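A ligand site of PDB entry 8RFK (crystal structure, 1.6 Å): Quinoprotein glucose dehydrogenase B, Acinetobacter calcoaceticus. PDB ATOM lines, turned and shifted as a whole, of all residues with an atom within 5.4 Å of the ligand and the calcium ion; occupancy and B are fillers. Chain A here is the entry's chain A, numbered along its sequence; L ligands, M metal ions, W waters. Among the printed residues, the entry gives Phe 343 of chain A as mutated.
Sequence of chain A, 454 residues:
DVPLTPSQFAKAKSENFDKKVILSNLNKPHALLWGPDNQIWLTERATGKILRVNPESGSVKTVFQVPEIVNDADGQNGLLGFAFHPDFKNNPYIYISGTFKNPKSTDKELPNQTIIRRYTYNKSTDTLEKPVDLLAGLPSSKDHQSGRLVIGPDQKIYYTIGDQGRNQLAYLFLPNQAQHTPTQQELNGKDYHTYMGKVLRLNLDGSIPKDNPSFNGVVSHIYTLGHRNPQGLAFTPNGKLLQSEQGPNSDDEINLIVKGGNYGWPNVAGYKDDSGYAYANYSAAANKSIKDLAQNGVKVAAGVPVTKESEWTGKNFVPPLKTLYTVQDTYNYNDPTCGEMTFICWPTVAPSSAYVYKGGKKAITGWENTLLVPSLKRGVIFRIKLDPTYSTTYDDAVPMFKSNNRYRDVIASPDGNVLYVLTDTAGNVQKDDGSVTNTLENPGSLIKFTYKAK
Water W2 binds the calcium ion, at 2.3 Å.
O of Pro 248 binds the calcium ion (2.4 Å).
O of Gly 247 is bound to the calcium ion (2.4 Å).
Water W1 binds the calcium ion, at 2.4 Å.
A nitrogen (N2) of the ligand is bound to the calcium ion.
An oxygen (O6) of the ligand binds the calcium ion, at 2.5 Å.
The calcium ion is bound by an oxygen (O9) of the ligand (2.5 Å).
The calcium ion has seven donor atoms within binding distance.
The side-chain hydroxyl of Thr 348 sits at hydrogen-bond distance from an oxygen (O8) of the ligand (3.1 Å).
NH2 of Arg 406 lies within salt-bridge range of O1 of the ligand (2.8 Å).
The side-chain amide nitrogen (NE2) of Gln 231 is in hydrogen-bond range of an oxygen (O5) of the ligand (2.8 Å).
The side-chain amide nitrogen (NE2) of Gln 246 lies within hydrogen-bond range of an oxygen (O5) of the ligand, 2.9 Å away.
An oxygen (O8) of the ligand is in salt-bridge range of the side-chain amino group of Lys 377 (3.0 Å).
An oxygen (O4) of the ligand is in salt-bridge range of the guanidinium group (NH2) of Arg 408.
O6 of the ligand sits close to NH1 of Arg 228.
Water W11 lies within hydrogen-bond range of O10 of the ligand (2.7 Å), O of Asn 428 (3.1 Å) and NH1 of Arg 406 (3.4 Å).
Water W3 bridges an oxygen (O4) of the ligand (3.0 Å) and the guanidinium group (NH1) of Arg 408 (3.5 Å).
Water W5 lies within hydrogen-bond range of a ring nitrogen (NE2) of His 144, an oxygen (O7) of the ligand and the guanidinium group of Arg 228.
Water W7 bridges an oxygen (O2) of the ligand (3.0 Å) and the guanidinium group of Arg 406 (3.4 Å).
Water W9 lies within hydrogen-bond range of the backbone NH of Asn 428 (3.0 Å), an oxygen (O10) of the ligand (3.0 Å) and the guanidinium group of Arg 406 (3.2 Å).
Water W10 lies within hydrogen-bond range of an oxygen (O4) of the ligand, the guanidinium group of Arg 406 and the guanidinium group of Arg 408.
Residues that only touch the ligand: Gln 76 (3.6 Å), His 144 (3.96 Å), Phe 343 (3.9 Å) and Leu 376 (3.4 Å).
Hydrophobic or aromatic side chains that line the ligand: Leu 376.
Within 4 Å of the ligand: Gln 76, His 144, Arg 228, Gln 231, Gln 246, Gly 247, Pro 248, Phe 343, Thr 348, Leu 376, Lys 377, Arg 406 and Arg 408.
The side-chain carboxylate of Asp 252 lies within hydrogen-bond range of the backbone NH of Gly 247 (2.7 Å).
The side-chain hydroxyl (OG1) of Thr 348 is in hydrogen-bond range of the side-chain amino group (NZ) of Lys 377, 2.8 Å away.
The side-chain amide nitrogen (NE2) of Gln 231 sits close to the side-chain amide nitrogen (ND2) of Asn 229 (3.4 Å).
NH1 of Arg 228 sits at hydrogen-bond distance from O of Gln 246 (3.0 Å).
N of Gln 246 is in hydrogen-bond range of O of Asn 229.
The side-chain amino group of Lys 377 sits at hydrogen-bond distance from the backbone carbonyl oxygen of Phe 343 (3.1 Å).
The side-chain carboxylate of Asp 424 lies within salt-bridge range of the guanidinium group of Arg 408.
The backbone carbonyl oxygen (O) of Ala 350 sits at hydrogen-bond distance from the backbone NH (N) of Leu 376 (3.0 Å).
The nearest printed residue that does not touch the calcium ion is Arg 228 (4.2 Å).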
ATOM      1  N   GLN A  76       5.946  33.824  -3.188  1.00  0.00           N
ATOM      2  CA  GLN A  76       4.882  32.837  -3.274  1.00  0.00           C
ATOM      3  C   GLN A  76       3.648  33.287  -2.502  1.00  0.00           C
ATOM      4  O   GLN A  76       2.816  32.450  -2.108  1.00  0.00           O
ATOM      5  CB  GLN A  76       5.380  31.489  -2.752  1.00  0.00           C
ATOM      6  CG  GLN A  76       6.514  30.867  -3.549  1.00  0.00           C
ATOM      7  CD  GLN A  76       7.850  30.983  -2.846  1.00  0.00           C
ATOM      8  OE1 GLN A  76       8.563  31.982  -2.998  1.00  0.00           O
ATOM      9  NE2 GLN A  76       8.185  29.970  -2.038  1.00  0.00           N
ATOM     10  N   HIS A 144       7.424  30.026   1.470  1.00  0.00           N
ATOM     11  CA  HIS A 144       6.824  28.915   2.221  1.00  0.00           C
ATOM     12  C   HIS A 144       5.554  29.368   2.939  1.00  0.00           C
ATOM     13  O   HIS A 144       5.434  29.278   4.164  1.00  0.00           O
ATOM     14  CB  HIS A 144       7.797  28.294   3.221  1.00  0.00           C
ATOM     15  CG  HIS A 144       9.093  27.830   2.607  1.00  0.00           C
ATOM     16  ND1 HIS A 144      10.186  27.482   3.371  1.00  0.00           N
ATOM     17  CD2 HIS A 144       9.471  27.709   1.319  1.00  0.00           C
ATOM     18  CE1 HIS A 144      11.179  27.151   2.566  1.00  0.00           C
ATOM     19  NE2 HIS A 144      10.779  27.279   1.314  1.00  0.00           N
ATOM     20  N   ARG A 228       7.383  22.378   7.122  1.00  0.00           N
ATOM     21  CA  ARG A 228       8.160  23.344   6.357  1.00  0.00           C
ATOM     22  C   ARG A 228       7.263  24.070   5.365  1.00  0.00           C
ATOM     23  O   ARG A 228       6.835  25.198   5.624  1.00  0.00           O
ATOM     24  CB  ARG A 228       9.340  22.636   5.674  1.00  0.00           C
ATOM     25  CG  ARG A 228      10.264  23.554   4.913  1.00  0.00           C
ATOM     26  CD  ARG A 228      11.390  22.777   4.226  1.00  0.00           C
ATOM     27  NE  ARG A 228      12.258  23.613   3.404  1.00  0.00           N
ATOM     28  CZ  ARG A 228      12.010  23.953   2.150  1.00  0.00           C
ATOM     29  NH1 ARG A 228      10.879  23.634   1.560  1.00  0.00           N
ATOM     30  NH2 ARG A 228      12.928  24.636   1.468  1.00  0.00           N
ATOM     31  N   ASN A 229       6.927  23.436   4.237  1.00  0.00           N
ATOM     32  CA  ASN A 229       6.017  24.039   3.252  1.00  0.00           C
ATOM     33  C   ASN A 229       5.000  22.998   2.802  1.00  0.00           C
ATOM     34  O   ASN A 229       5.129  22.387   1.732  1.00  0.00           O
ATOM     35  CB  ASN A 229       6.785  24.604   2.057  1.00  0.00           C
ATOM     36  CG  ASN A 229       5.882  25.381   1.107  1.00  0.00           C
ATOM     37  OD1 ASN A 229       4.775  25.753   1.475  1.00  0.00           O
ATOM     38  ND2 ASN A 229       6.362  25.639  -0.105  1.00  0.00           N
ATOM     39  N   GLN A 231       2.046  22.106   1.013  1.00  0.00           N
ATOM     40  CA  GLN A 231       1.107  22.652   0.030  1.00  0.00           C
ATOM     41  C   GLN A 231      -0.020  21.699  -0.336  1.00  0.00           C
ATOM     42  O   GLN A 231      -0.970  22.127  -0.995  1.00  0.00           O
ATOM     43  CB  GLN A 231       1.871  23.043  -1.242  1.00  0.00           C
ATOM     44  CG  GLN A 231       2.771  24.261  -1.054  1.00  0.00           C
ATOM     45  CD  GLN A 231       3.519  24.629  -2.315  1.00  0.00           C
ATOM     46  OE1 GLN A 231       3.711  23.799  -3.201  1.00  0.00           O
ATOM     47  NE2 GLN A 231       3.915  25.888  -2.431  1.00  0.00           N
ATOM     48  N   GLN A 246       6.955  20.197   0.988  1.00  0.00           N
ATOM     49  CA  GLN A 246       8.271  20.393   0.373  1.00  0.00           C
ATOM     50  C   GLN A 246       9.352  20.424   1.448  1.00  0.00           C
ATOM     51  O   GLN A 246       9.261  21.197   2.403  1.00  0.00           O
ATOM     52  CB  GLN A 246       8.323  21.679  -0.448  1.00  0.00           C
ATOM     53  CG  GLN A 246       7.236  21.815  -1.490  1.00  0.00           C
ATOM     54  CD  GLN A 246       7.613  22.707  -2.659  1.00  0.00           C
ATOM     55  OE1 GLN A 246       8.789  22.986  -2.894  1.00  0.00           O
ATOM     56  NE2 GLN A 246       6.605  23.194  -3.367  1.00  0.00           N
ATOM     57  N   GLY A 247      10.364  19.576   1.275  1.00  0.00           N
ATOM     58  CA  GLY A 247      11.556  19.613   2.087  1.00  0.00           C
ATOM     59  C   GLY A 247      12.611  20.504   1.465  1.00  0.00           C
ATOM     60  O   GLY A 247      12.399  21.138   0.421  1.00  0.00           O
ATOM     61  N   PRO A 248      13.787  20.585   2.102  1.00  0.00           N
ATOM     62  CA  PRO A 248      14.868  21.455   1.606  1.00  0.00           C
ATOM     63  C   PRO A 248      15.596  20.891   0.384  1.00  0.00           C
ATOM     64  O   PRO A 248      14.998  20.865  -0.693  1.00  0.00           O
ATOM     65  CB  PRO A 248      15.778  21.582   2.849  1.00  0.00           C
ATOM     66  CG  PRO A 248      15.626  20.239   3.516  1.00  0.00           C
ATOM     67  CD  PRO A 248      14.148  19.910   3.370  1.00  0.00           C
ATOM     68  N   ASN A 249      16.873  20.466   0.481  1.00  0.00           N
ATOM     69  CA  ASN A 249      17.533  19.833  -0.658  1.00  0.00           C
ATOM     70  C   ASN A 249      17.084  18.384  -0.852  1.00  0.00           C
ATOM     71  O   ASN A 249      17.534  17.738  -1.801  1.00  0.00           O
ATOM     72  CB  ASN A 249      19.064  19.792  -0.539  1.00  0.00           C
ATOM     73  CG  ASN A 249      19.701  21.141  -0.332  1.00  0.00           C
ATOM     74  OD1 ASN A 249      19.058  22.127  -0.007  1.00  0.00           O
ATOM     75  ND2 ASN A 249      21.007  21.192  -0.551  1.00  0.00           N
ATOM     76  N   ASP A 252      11.269  15.797   0.468  1.00  0.00           N
ATOM     77  CA  ASP A 252       9.841  16.071   0.312  1.00  0.00           C
ATOM     78  C   ASP A 252       9.072  14.919   0.952  1.00  0.00           C
ATOM     79  O   ASP A 252       9.560  13.781   0.995  1.00  0.00           O
ATOM     80  CB  ASP A 252       9.452  16.227  -1.154  1.00  0.00           C
ATOM     81  CG  ASP A 252      10.131  17.418  -1.840  1.00  0.00           C
ATOM     82  OD1 ASP A 252      10.410  18.440  -1.178  1.00  0.00           O
ATOM     83  OD2 ASP A 252      10.340  17.333  -3.059  1.00  0.00           O
ATOM     84  N   PHE A 343      20.998  22.214  -8.547  1.00  0.00           N
ATOM     85  CA  PHE A 343      19.763  22.002  -7.806  1.00  0.00           C
ATOM     86  C   PHE A 343      18.762  21.141  -8.562  1.00  0.00           C
ATOM     87  O   PHE A 343      17.906  20.509  -7.931  1.00  0.00           O
ATOM     88  CB  PHE A 343      19.157  23.362  -7.454  1.00  0.00           C
ATOM     89  CG  PHE A 343      18.258  23.921  -8.516  1.00  0.00           C
ATOM     90  CD1 PHE A 343      16.961  23.464  -8.691  1.00  0.00           C
ATOM     91  CD2 PHE A 343      18.734  24.875  -9.387  1.00  0.00           C
ATOM     92  CE1 PHE A 343      16.151  23.973  -9.684  1.00  0.00           C
ATOM     93  CE2 PHE A 343      17.934  25.385 -10.385  1.00  0.00           C
ATOM     94  CZ  PHE A 343      16.648  24.937 -10.532  1.00  0.00           C
ATOM     95  N   TRP A 346      18.854  17.668  -7.420  1.00  0.00           N
ATOM     96  CA  TRP A 346      18.655  17.404  -6.001  1.00  0.00           C
ATOM     97  C   TRP A 346      17.576  16.350  -5.815  1.00  0.00           C
ATOM     98  O   TRP A 346      16.636  16.273  -6.633  1.00  0.00           O
ATOM     99  CB  TRP A 346      18.271  18.687  -5.267  1.00  0.00           C
ATOM    100  CG  TRP A 346      19.412  19.598  -4.994  1.00  0.00           C
ATOM    101  CD1 TRP A 346      20.719  19.400  -5.313  1.00  0.00           C
ATOM    102  CD2 TRP A 346      19.339  20.868  -4.353  1.00  0.00           C
ATOM    103  NE1 TRP A 346      21.478  20.467  -4.897  1.00  0.00           N
ATOM    104  CE2 TRP A 346      20.648  21.391  -4.314  1.00  0.00           C
ATOM    105  CE3 TRP A 346      18.297  21.627  -3.819  1.00  0.00           C
ATOM    106  CZ2 TRP A 346      20.942  22.622  -3.739  1.00  0.00           C
ATOM    107  CZ3 TRP A 346      18.588  22.851  -3.252  1.00  0.00           C
ATOM    108  CH2 TRP A 346      19.896  23.333  -3.221  1.00  0.00           C
ATOM    109  N   THR A 348      14.687  15.821  -4.757  1.00  0.00           N
ATOM    110  CA  THR A 348      13.389  16.389  -4.424  1.00  0.00           C
ATOM    111  C   THR A 348      12.521  16.392  -5.679  1.00  0.00           C
ATOM    112  O   THR A 348      13.008  16.213  -6.806  1.00  0.00           O
ATOM    113  CB  THR A 348      13.510  17.817  -3.891  1.00  0.00           C
ATOM    114  OG1 THR A 348      14.239  18.602  -4.855  1.00  0.00           O
ATOM    115  CG2 THR A 348      14.230  17.832  -2.548  1.00  0.00           C
ATOM    116  N   ALA A 350       9.488  18.669  -5.330  1.00  0.00           N
ATOM    117  CA  ALA A 350       8.734  19.905  -5.073  1.00  0.00           C
ATOM    118  C   ALA A 350       7.243  19.666  -5.285  1.00  0.00           C
ATOM    119  O   ALA A 350       6.640  20.244  -6.204  1.00  0.00           O
ATOM    120  CB  ALA A 350       9.236  21.041  -5.963  1.00  0.00           C
ATOM    121  N   LEU A 376       6.354  20.168  -9.237  1.00  0.00           N
ATOM    122  CA  LEU A 376       6.774  21.374  -9.934  1.00  0.00           C
ATOM    123  C   LEU A 376       8.080  21.143 -10.693  1.00  0.00           C
ATOM    124  O   LEU A 376       8.206  21.497 -11.873  1.00  0.00           O
ATOM    125  CB  LEU A 376       6.942  22.530  -8.943  1.00  0.00           C
ATOM    126  CG  LEU A 376       5.689  22.976  -8.187  1.00  0.00           C
ATOM    127  CD1 LEU A 376       6.064  23.874  -7.014  1.00  0.00           C
ATOM    128  CD2 LEU A 376       4.734  23.699  -9.113  1.00  0.00           C
ATOM    129  N   LYS A 377       9.058  20.526 -10.018  1.00  0.00           N
ATOM    130  CA  LYS A 377      10.410  20.500 -10.556  1.00  0.00           C
ATOM    131  C   LYS A 377      10.615  19.407 -11.590  1.00  0.00           C
ATOM    132  O   LYS A 377      11.475  19.543 -12.463  1.00  0.00           O
ATOM    133  CB  LYS A 377      11.420  20.321  -9.422  1.00  0.00           C
ATOM    134  CG  LYS A 377      12.847  20.197  -9.902  1.00  0.00           C
ATOM    135  CD  LYS A 377      13.840  20.320  -8.769  1.00  0.00           C
ATOM    136  CE  LYS A 377      13.983  19.015  -8.028  1.00  0.00           C
ATOM    137  NZ  LYS A 377      15.337  18.917  -7.458  1.00  0.00           N
ATOM    138  N   ARG A 406       5.521  22.961 -14.991  1.00  0.00           N
ATOM    139  CA  ARG A 406       5.489  22.974 -13.537  1.00  0.00           C
ATOM    140  C   ARG A 406       4.044  22.721 -13.116  1.00  0.00           C
ATOM    141  O   ARG A 406       3.219  23.635 -13.153  1.00  0.00           O
ATOM    142  CB  ARG A 406       6.008  24.301 -13.010  1.00  0.00           C
ATOM    143  CG  ARG A 406       7.512  24.453 -13.097  1.00  0.00           C
ATOM    144  CD  ARG A 406       7.918  25.887 -12.807  1.00  0.00           C
ATOM    145  NE  ARG A 406       7.641  26.246 -11.413  1.00  0.00           N
ATOM    146  CZ  ARG A 406       8.394  25.889 -10.381  1.00  0.00           C
ATOM    147  NH1 ARG A 406       9.475  25.137 -10.537  1.00  0.00           N
ATOM    148  NH2 ARG A 406       8.035  26.280  -9.165  1.00  0.00           N
ATOM    149  N   ARG A 408       0.971  22.356 -10.846  1.00  0.00           N
ATOM    150  CA  ARG A 408       0.652  23.122  -9.643  1.00  0.00           C
ATOM    151  C   ARG A 408      -0.532  22.560  -8.878  1.00  0.00           C
ATOM    152  O   ARG A 408      -0.588  22.727  -7.653  1.00  0.00           O
ATOM    153  CB  ARG A 408       0.371  24.587 -10.039  1.00  0.00           C
ATOM    154  CG  ARG A 408      -0.077  25.521  -8.929  1.00  0.00           C
ATOM    155  CD  ARG A 408       0.891  25.609  -7.759  1.00  0.00           C
ATOM    156  NE  ARG A 408       2.183  26.185  -8.114  1.00  0.00           N
ATOM    157  CZ  ARG A 408       3.179  26.355  -7.258  1.00  0.00           C
ATOM    158  NH1 ARG A 408       3.062  26.041  -5.981  1.00  0.00           N
ATOM    159  NH2 ARG A 408       4.326  26.876  -7.697  1.00  0.00           N
ATOM    160  N   ASP A 424       2.207  26.265 -13.806  1.00  0.00           N
ATOM    161  CA  ASP A 424       2.745  27.560 -13.436  1.00  0.00           C
ATOM    162  C   ASP A 424       2.995  28.416 -14.671  1.00  0.00           C
ATOM    163  O   ASP A 424       3.200  27.917 -15.780  1.00  0.00           O
ATOM    164  CB  ASP A 424       4.063  27.431 -12.682  1.00  0.00           C
ATOM    165  CG  ASP A 424       3.883  27.149 -11.203  1.00  0.00           C
ATOM    166  OD1 ASP A 424       2.733  27.051 -10.718  1.00  0.00           O
ATOM    167  OD2 ASP A 424       4.934  27.054 -10.523  1.00  0.00           O
ATOM    168  N   ASN A 428      11.540  27.012 -13.245  1.00  0.00           N
ATOM    169  CA  ASN A 428      12.421  25.977 -13.777  1.00  0.00           C
ATOM    170  C   ASN A 428      11.758  24.610 -13.706  1.00  0.00           C
ATOM    171  O   ASN A 428      10.960  24.326 -12.810  1.00  0.00           O
ATOM    172  CB  ASN A 428      13.738  25.926 -13.016  1.00  0.00           C
ATOM    173  CG  ASN A 428      14.452  27.263 -13.004  1.00  0.00           C
ATOM    174  OD1 ASN A 428      14.803  27.769 -11.931  1.00  0.00           O
ATOM    175  ND2 ASN A 428      14.671  27.829 -14.173  1.00  0.00           N
HETATM  176  C1  LIG L   1      11.639  24.327  -6.166  1.00  0.00           C
HETATM  177  C2  LIG L   1      12.617  23.341  -6.189  1.00  0.00           C
HETATM  178  C3  LIG L   1      13.032  22.810  -4.976  1.00  0.00           C
HETATM  179  C4  LIG L   1      11.614  24.174  -3.772  1.00  0.00           C
HETATM  180  C5  LIG L   1      10.126  25.883  -4.978  1.00  0.00           C
HETATM  181  C6  LIG L   1       8.972  27.819  -5.326  1.00  0.00           C
HETATM  182  C7  LIG L   1      11.533  27.953  -5.702  1.00  0.00           C
HETATM  183  C8  LIG L   1      11.130  24.537  -2.376  1.00  0.00           C
HETATM  184  C9  LIG L   1      14.082  21.706  -4.951  1.00  0.00           C
HETATM  185  C10 LIG L   1       8.068  26.835  -4.988  1.00  0.00           C
HETATM  186  C11 LIG L   1      10.270  27.229  -5.324  1.00  0.00           C
HETATM  187  C12 LIG L   1       6.575  26.858  -4.883  1.00  0.00           C
HETATM  188  C13 LIG L   1      11.128  24.850  -7.493  1.00  0.00           C
HETATM  189  C14 LIG L   1      11.104  24.785  -4.942  1.00  0.00           C
HETATM  190  N1  LIG L   1       8.778  25.671  -4.776  1.00  0.00           N
HETATM  191  N2  LIG L   1      12.556  23.210  -3.798  1.00  0.00           N
HETATM  192  O1  LIG L   1       9.908  24.853  -7.684  1.00  0.00           O
HETATM  193  O2  LIG L   1      11.416  29.076  -6.260  1.00  0.00           O
HETATM  194  O3  LIG L   1      12.633  27.391  -5.453  1.00  0.00           O
HETATM  195  O4  LIG L   1       5.990  27.820  -5.402  1.00  0.00           O
HETATM  196  O5  LIG L   1       6.023  25.905  -4.300  1.00  0.00           O
HETATM  197  O6  LIG L   1      11.481  23.767  -1.429  1.00  0.00           O
HETATM  198  O7  LIG L   1      10.439  25.579  -2.247  1.00  0.00           O
HETATM  199  O8  LIG L   1      14.678  21.443  -6.018  1.00  0.00           O
HETATM  200  O9  LIG L   1      14.262  21.108  -3.855  1.00  0.00           O
HETATM  201  O10 LIG L   1      11.982  25.244  -8.325  1.00  0.00           O
HETATM  202 CA    CA M   1      13.093  21.939  -1.780  1.00  0.00          CA
HETATM  203  O   HOH W   1      11.237  20.557  -2.564  1.00  0.00           O
HETATM  204  O   HOH W   2      14.419  23.858  -1.514  1.00  0.00           O
HETATM  205  O   HOH W   3       3.526  29.455  -5.401  1.00  0.00           O
HETATM  206  O   HOH W   4      14.016  26.141  -2.828  1.00  0.00           O
HETATM  207  O   HOH W   5      12.693  26.851  -0.743  1.00  0.00           O
HETATM  208  O   HOH W   6      10.846  28.415  -1.982  1.00  0.00           O
HETATM  209  O   HOH W   7       9.652  29.191  -8.698  1.00  0.00           O
HETATM  210  O   HOH W   8      14.253  29.306  -3.720  1.00  0.00           O
HETATM  211  O   HOH W   9      11.575  27.497 -10.306  1.00  0.00           O
HETATM  212  O   HOH W  10       6.792  28.958  -8.122  1.00  0.00           O
HETATM  213  O   HOH W  11      12.378  23.410 -10.260  1.00  0.00           O
